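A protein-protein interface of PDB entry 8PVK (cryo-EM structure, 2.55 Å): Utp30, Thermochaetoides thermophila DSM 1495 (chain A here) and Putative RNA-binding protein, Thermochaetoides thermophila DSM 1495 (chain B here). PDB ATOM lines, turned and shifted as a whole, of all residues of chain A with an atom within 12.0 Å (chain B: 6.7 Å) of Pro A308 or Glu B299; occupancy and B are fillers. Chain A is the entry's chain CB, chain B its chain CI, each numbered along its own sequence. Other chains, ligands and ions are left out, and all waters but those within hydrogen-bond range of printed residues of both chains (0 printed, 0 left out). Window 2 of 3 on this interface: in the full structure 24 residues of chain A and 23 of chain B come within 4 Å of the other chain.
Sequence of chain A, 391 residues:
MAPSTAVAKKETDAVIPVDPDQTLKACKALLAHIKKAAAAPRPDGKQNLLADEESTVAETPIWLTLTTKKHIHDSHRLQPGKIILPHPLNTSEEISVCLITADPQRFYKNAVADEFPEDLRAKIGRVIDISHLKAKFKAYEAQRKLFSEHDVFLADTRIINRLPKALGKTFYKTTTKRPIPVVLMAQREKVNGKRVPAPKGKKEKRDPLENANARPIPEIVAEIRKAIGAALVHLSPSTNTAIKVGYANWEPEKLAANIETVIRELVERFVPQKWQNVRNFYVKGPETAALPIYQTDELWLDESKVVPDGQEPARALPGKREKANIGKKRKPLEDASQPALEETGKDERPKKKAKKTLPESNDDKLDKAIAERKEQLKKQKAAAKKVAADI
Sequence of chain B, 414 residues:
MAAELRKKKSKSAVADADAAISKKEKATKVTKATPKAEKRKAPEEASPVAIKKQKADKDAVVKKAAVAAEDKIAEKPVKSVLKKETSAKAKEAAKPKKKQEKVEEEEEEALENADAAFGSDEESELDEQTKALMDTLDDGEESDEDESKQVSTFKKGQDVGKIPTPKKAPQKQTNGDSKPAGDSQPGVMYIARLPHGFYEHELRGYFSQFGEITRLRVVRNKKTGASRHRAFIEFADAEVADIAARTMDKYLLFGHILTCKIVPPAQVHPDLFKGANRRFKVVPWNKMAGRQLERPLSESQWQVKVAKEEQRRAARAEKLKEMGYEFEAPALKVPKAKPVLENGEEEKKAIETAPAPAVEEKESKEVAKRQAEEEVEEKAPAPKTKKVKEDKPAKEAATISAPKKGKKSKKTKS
Among the printed residues, pairs that only touch across the chains: Trp A300 with Trp B302 (3.4 Å), Pro A308 with Glu B299 (3.4 Å), Leu A299 with Trp B302 (3.4 Å), Trp A300 with Pro B335 (3.6 Å) and Lys A305 with Leu B297 (3.996 Å).
NE2 of Gln B303 is in hydrogen-bond range of O of Glu B299 (2.7 Å).
The backbone carbonyl oxygen of Val A307 sits close to the side-chain carboxylate of Glu B299.
Of chain B, only Glu B299 (3.4 Å) comes within 4 Å of Pro A308.
Glu B299 touches just these residues of chain A: Val A307 and Pro A308.
No residue of chain A comes within 4 Å of Ser B300.
No residue of chain A comes within 4 Å of Gln B303.
Printed residues of chain B within 4 Å of Lys A305: Leu B297 (3.996 Å).
Printed residues of chain B within 4 Å of Val A307: Glu B299 (2.9 Å).
Printed residues of chain A within 4 Å of Leu B297: Lys A305 (3.996 Å).
Of the printed residues of chain B, Leu A299 touches Trp B302.
The nearest residue of chain B that does not touch Pro A308 is Ser B298 (5.4 Å).
The nearest residue of chain A that does not touch Glu B299 is Val A306 (4.3 Å).
The nearest printed residue of chain A that does not touch Leu B297 is Val A307 (4.1 Å).
Of the 9 printed residues of chain A, 5 touch a printed residue of chain B.
Hydrophobic or aromatic side chains of chain B within 4 Å of the printed part of chain A: Trp B302 and Pro B335.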
ATOM      1  N   LEU A 299      11.971  17.841  13.289  1.00  0.00           N
ATOM      2  CA  LEU A 299      11.600  19.203  12.935  1.00  0.00           C
ATOM      3  C   LEU A 299      11.192  19.348  11.474  1.00  0.00           C
ATOM      4  O   LEU A 299      10.762  20.435  11.075  1.00  0.00           O
ATOM      5  CB  LEU A 299      12.745  20.171  13.250  1.00  0.00           C
ATOM      6  CG  LEU A 299      13.243  20.203  14.695  1.00  0.00           C
ATOM      7  CD1 LEU A 299      14.476  21.091  14.819  1.00  0.00           C
ATOM      8  CD2 LEU A 299      12.140  20.649  15.648  1.00  0.00           C
ATOM      9  N   TRP A 300      11.314  18.296  10.669  1.00  0.00           N
ATOM     10  CA  TRP A 300      10.806  18.320   9.305  1.00  0.00           C
ATOM     11  C   TRP A 300       9.359  17.846   9.274  1.00  0.00           C
ATOM     12  O   TRP A 300       8.880  17.185  10.199  1.00  0.00           O
ATOM     13  CB  TRP A 300      11.642  17.458   8.353  1.00  0.00           C
ATOM     14  CG  TRP A 300      12.093  16.132   8.903  1.00  0.00           C
ATOM     15  CD1 TRP A 300      11.302  15.071   9.239  1.00  0.00           C
ATOM     16  CD2 TRP A 300      13.446  15.678   9.046  1.00  0.00           C
ATOM     17  NE1 TRP A 300      12.075  14.016   9.658  1.00  0.00           N
ATOM     18  CE2 TRP A 300      13.396  14.360   9.539  1.00  0.00           C
ATOM     19  CE3 TRP A 300      14.696  16.268   8.829  1.00  0.00           C
ATOM     20  CZ2 TRP A 300      14.543  13.623   9.820  1.00  0.00           C
ATOM     21  CZ3 TRP A 300      15.835  15.537   9.113  1.00  0.00           C
ATOM     22  CH2 TRP A 300      15.750  14.228   9.602  1.00  0.00           C
ATOM     23  N   ASP A 302       7.986  15.824   6.768  1.00  0.00           N
ATOM     24  CA  ASP A 302       8.035  14.411   6.405  1.00  0.00           C
ATOM     25  C   ASP A 302       9.361  14.145   5.699  1.00  0.00           C
ATOM     26  O   ASP A 302      10.275  14.975   5.727  1.00  0.00           O
ATOM     27  CB  ASP A 302       6.835  14.018   5.534  1.00  0.00           C
ATOM     28  CG  ASP A 302       6.634  14.951   4.358  1.00  0.00           C
ATOM     29  OD1 ASP A 302       7.297  16.009   4.310  1.00  0.00           O
ATOM     30  OD2 ASP A 302       5.813  14.625   3.475  1.00  0.00           O
ATOM     31  N   GLU A 303       9.466  12.979   5.061  1.00  0.00           N
ATOM     32  CA  GLU A 303      10.669  12.622   4.322  1.00  0.00           C
ATOM     33  C   GLU A 303      10.696  13.196   2.912  1.00  0.00           C
ATOM     34  O   GLU A 303      11.741  13.128   2.256  1.00  0.00           O
ATOM     35  CB  GLU A 303      10.818  11.100   4.255  1.00  0.00           C
ATOM     36  CG  GLU A 303       9.815  10.416   3.341  1.00  0.00           C
ATOM     37  CD  GLU A 303       8.566   9.963   4.072  1.00  0.00           C
ATOM     38  OE1 GLU A 303       8.339  10.423   5.211  1.00  0.00           O
ATOM     39  OE2 GLU A 303       7.813   9.144   3.508  1.00  0.00           O
ATOM     40  N   SER A 304       9.582  13.752   2.427  1.00  0.00           N
ATOM     41  CA  SER A 304       9.575  14.361   1.101  1.00  0.00           C
ATOM     42  C   SER A 304      10.308  15.695   1.078  1.00  0.00           C
ATOM     43  O   SER A 304      10.664  16.174  -0.004  1.00  0.00           O
ATOM     44  CB  SER A 304       8.139  14.546   0.609  1.00  0.00           C
ATOM     45  OG  SER A 304       7.445  15.495   1.399  1.00  0.00           O
ATOM     46  N   LYS A 305      10.538  16.305   2.243  1.00  0.00           N
ATOM     47  CA  LYS A 305      11.344  17.515   2.315  1.00  0.00           C
ATOM     48  C   LYS A 305      12.836  17.218   2.236  1.00  0.00           C
ATOM     49  O   LYS A 305      13.635  18.151   2.105  1.00  0.00           O
ATOM     50  CB  LYS A 305      11.041  18.275   3.607  1.00  0.00           C
ATOM     51  CG  LYS A 305       9.588  18.695   3.772  1.00  0.00           C
ATOM     52  CD  LYS A 305       9.222  19.832   2.832  1.00  0.00           C
ATOM     53  CE  LYS A 305       8.142  19.416   1.848  1.00  0.00           C
ATOM     54  NZ  LYS A 305       7.725  20.549   0.975  1.00  0.00           N
ATOM     55  N   VAL A 306      13.226  15.948   2.312  1.00  0.00           N
ATOM     56  CA  VAL A 306      14.634  15.568   2.323  1.00  0.00           C
ATOM     57  C   VAL A 306      15.139  15.546   0.883  1.00  0.00           C
ATOM     58  O   VAL A 306      14.684  14.741   0.066  1.00  0.00           O
ATOM     59  CB  VAL A 306      14.843  14.211   3.002  1.00  0.00           C
ATOM     60  CG1 VAL A 306      16.303  13.792   2.912  1.00  0.00           C
ATOM     61  CG2 VAL A 306      14.386  14.268   4.452  1.00  0.00           C
ATOM     62  N   VAL A 307      16.079  16.432   0.572  1.00  0.00           N
ATOM     63  CA  VAL A 307      16.718  16.455  -0.741  1.00  0.00           C
ATOM     64  C   VAL A 307      18.187  16.837  -0.567  1.00  0.00           C
ATOM     65  O   VAL A 307      18.504  17.813   0.132  1.00  0.00           O
ATOM     66  CB  VAL A 307      15.961  17.382  -1.714  1.00  0.00           C
ATOM     67  CG1 VAL A 307      15.802  18.798  -1.155  1.00  0.00           C
ATOM     68  CG2 VAL A 307      16.647  17.414  -3.073  1.00  0.00           C
ATOM     69  N   PRO A 308      19.125  16.067  -1.138  1.00  0.00           N
ATOM     70  CA  PRO A 308      20.552  16.375  -1.006  1.00  0.00           C
ATOM     71  C   PRO A 308      21.086  17.202  -2.172  1.00  0.00           C
ATOM     72  O   PRO A 308      22.041  17.952  -1.976  1.00  0.00           O
ATOM     73  CB  PRO A 308      21.209  14.989  -0.975  1.00  0.00           C
ATOM     74  CG  PRO A 308      20.155  14.012  -1.482  1.00  0.00           C
ATOM     75  CD  PRO A 308      18.910  14.780  -1.817  1.00  0.00           C
ATOM     76  N   LEU B 297      14.505  22.350   1.539  1.00  0.00           N
ATOM     77  CA  LEU B 297      15.776  23.039   1.715  1.00  0.00           C
ATOM     78  C   LEU B 297      16.849  22.031   2.117  1.00  0.00           C
ATOM     79  O   LEU B 297      16.566  20.855   2.359  1.00  0.00           O
ATOM     80  CB  LEU B 297      15.655  24.189   2.735  1.00  0.00           C
ATOM     81  CG  LEU B 297      15.514  23.959   4.243  1.00  0.00           C
ATOM     82  CD1 LEU B 297      15.806  25.250   4.997  1.00  0.00           C
ATOM     83  CD2 LEU B 297      14.127  23.452   4.614  1.00  0.00           C
ATOM     84  N   SER B 298      18.089  22.509   2.184  1.00  0.00           N
ATOM     85  CA  SER B 298      19.260  21.643   2.154  1.00  0.00           C
ATOM     86  C   SER B 298      19.765  21.284   3.555  1.00  0.00           C
ATOM     87  O   SER B 298      19.360  21.855   4.572  1.00  0.00           O
ATOM     88  CB  SER B 298      20.381  22.300   1.347  1.00  0.00           C
ATOM     89  OG  SER B 298      19.971  22.555   0.016  1.00  0.00           O
ATOM     90  N   GLU B 299      20.696  20.324   3.581  1.00  0.00           N
ATOM     91  CA  GLU B 299      21.160  19.727   4.829  1.00  0.00           C
ATOM     92  C   GLU B 299      22.095  20.630   5.627  1.00  0.00           C
ATOM     93  O   GLU B 299      22.107  20.547   6.858  1.00  0.00           O
ATOM     94  CB  GLU B 299      21.849  18.388   4.551  1.00  0.00           C
ATOM     95  CG  GLU B 299      20.901  17.251   4.190  1.00  0.00           C
ATOM     96  CD  GLU B 299      20.527  17.228   2.723  1.00  0.00           C
ATOM     97  OE1 GLU B 299      21.061  18.054   1.953  1.00  0.00           O
ATOM     98  OE2 GLU B 299      19.697  16.377   2.338  1.00  0.00           O
ATOM     99  N   SER B 300      22.896  21.476   4.975  1.00  0.00           N
ATOM    100  CA  SER B 300      23.803  22.346   5.723  1.00  0.00           C
ATOM    101  C   SER B 300      23.026  23.389   6.522  1.00  0.00           C
ATOM    102  O   SER B 300      23.239  23.567   7.734  1.00  0.00           O
ATOM    103  CB  SER B 300      24.793  23.019   4.773  1.00  0.00           C
ATOM    104  OG  SER B 300      25.648  23.901   5.480  1.00  0.00           O
ATOM    105  N   GLN B 301      22.083  24.065   5.867  1.00  0.00           N
ATOM    106  CA  GLN B 301      21.194  24.928   6.622  1.00  0.00           C
ATOM    107  C   GLN B 301      20.231  24.139   7.496  1.00  0.00           C
ATOM    108  O   GLN B 301      19.673  24.717   8.426  1.00  0.00           O
ATOM    109  CB  GLN B 301      20.425  25.877   5.698  1.00  0.00           C
ATOM    110  CG  GLN B 301      19.494  25.213   4.715  1.00  0.00           C
ATOM    111  CD  GLN B 301      20.083  25.153   3.326  1.00  0.00           C
ATOM    112  OE1 GLN B 301      21.286  24.960   3.156  1.00  0.00           O
ATOM    113  NE2 GLN B 301      19.238  25.334   2.318  1.00  0.00           N
ATOM    114  N   TRP B 302      20.055  22.830   7.264  1.00  0.00           N
ATOM    115  CA  TRP B 302      19.343  22.024   8.256  1.00  0.00           C
ATOM    116  C   TRP B 302      20.146  21.890   9.546  1.00  0.00           C
ATOM    117  O   TRP B 302      19.577  21.914  10.642  1.00  0.00           O
ATOM    118  CB  TRP B 302      19.014  20.631   7.726  1.00  0.00           C
ATOM    119  CG  TRP B 302      18.228  19.888   8.745  1.00  0.00           C
ATOM    120  CD1 TRP B 302      18.674  18.918   9.593  1.00  0.00           C
ATOM    121  CD2 TRP B 302      16.851  20.090   9.051  1.00  0.00           C
ATOM    122  NE1 TRP B 302      17.649  18.496  10.407  1.00  0.00           N
ATOM    123  CE2 TRP B 302      16.517  19.200  10.089  1.00  0.00           C
ATOM    124  CE3 TRP B 302      15.861  20.934   8.540  1.00  0.00           C
ATOM    125  CZ2 TRP B 302      15.236  19.134  10.627  1.00  0.00           C
ATOM    126  CZ3 TRP B 302      14.595  20.865   9.070  1.00  0.00           C
ATOM    127  CH2 TRP B 302      14.290  19.971  10.100  1.00  0.00           C
ATOM    128  N   GLN B 303      21.463  21.695   9.436  1.00  0.00           N
ATOM    129  CA  GLN B 303      22.286  21.637  10.643  1.00  0.00           C
ATOM    130  C   GLN B 303      22.293  22.979  11.365  1.00  0.00           C
ATOM    131  O   GLN B 303      22.221  23.021  12.598  1.00  0.00           O
ATOM    132  CB  GLN B 303      23.721  21.191  10.332  1.00  0.00           C
ATOM    133  CG  GLN B 303      23.903  19.987   9.398  1.00  0.00           C
ATOM    134  CD  GLN B 303      22.869  18.881   9.577  1.00  0.00           C
ATOM    135  OE1 GLN B 303      22.593  18.434  10.693  1.00  0.00           O
ATOM    136  NE2 GLN B 303      22.297  18.430   8.466  1.00  0.00           N
ATOM    137  N   VAL B 304      22.356  24.082  10.613  1.00  0.00           N
ATOM    138  CA  VAL B 304      22.289  25.411  11.235  1.00  0.00           C
ATOM    139  C   VAL B 304      20.921  25.634  11.890  1.00  0.00           C
ATOM    140  O   VAL B 304      20.822  26.159  13.009  1.00  0.00           O
ATOM    141  CB  VAL B 304      22.617  26.501  10.198  1.00  0.00           C
ATOM    142  CG1 VAL B 304      22.503  27.889  10.813  1.00  0.00           C
ATOM    143  CG2 VAL B 304      24.010  26.278   9.626  1.00  0.00           C
ATOM    144  N   PRO B 335      19.828  14.211  10.192  1.00  0.00           N
ATOM    145  CA  PRO B 335      19.797  13.330   9.022  1.00  0.00           C
ATOM    146  C   PRO B 335      21.197  12.951   8.563  1.00  0.00           C
ATOM    147  O   PRO B 335      21.490  13.095   7.377  1.00  0.00           O
ATOM    148  CB  PRO B 335      19.087  14.179   7.964  1.00  0.00           C
ATOM    149  CG  PRO B 335      19.402  15.565   8.348  1.00  0.00           C
ATOM    150  CD  PRO B 335      19.402  15.577   9.848  1.00  0.00           C
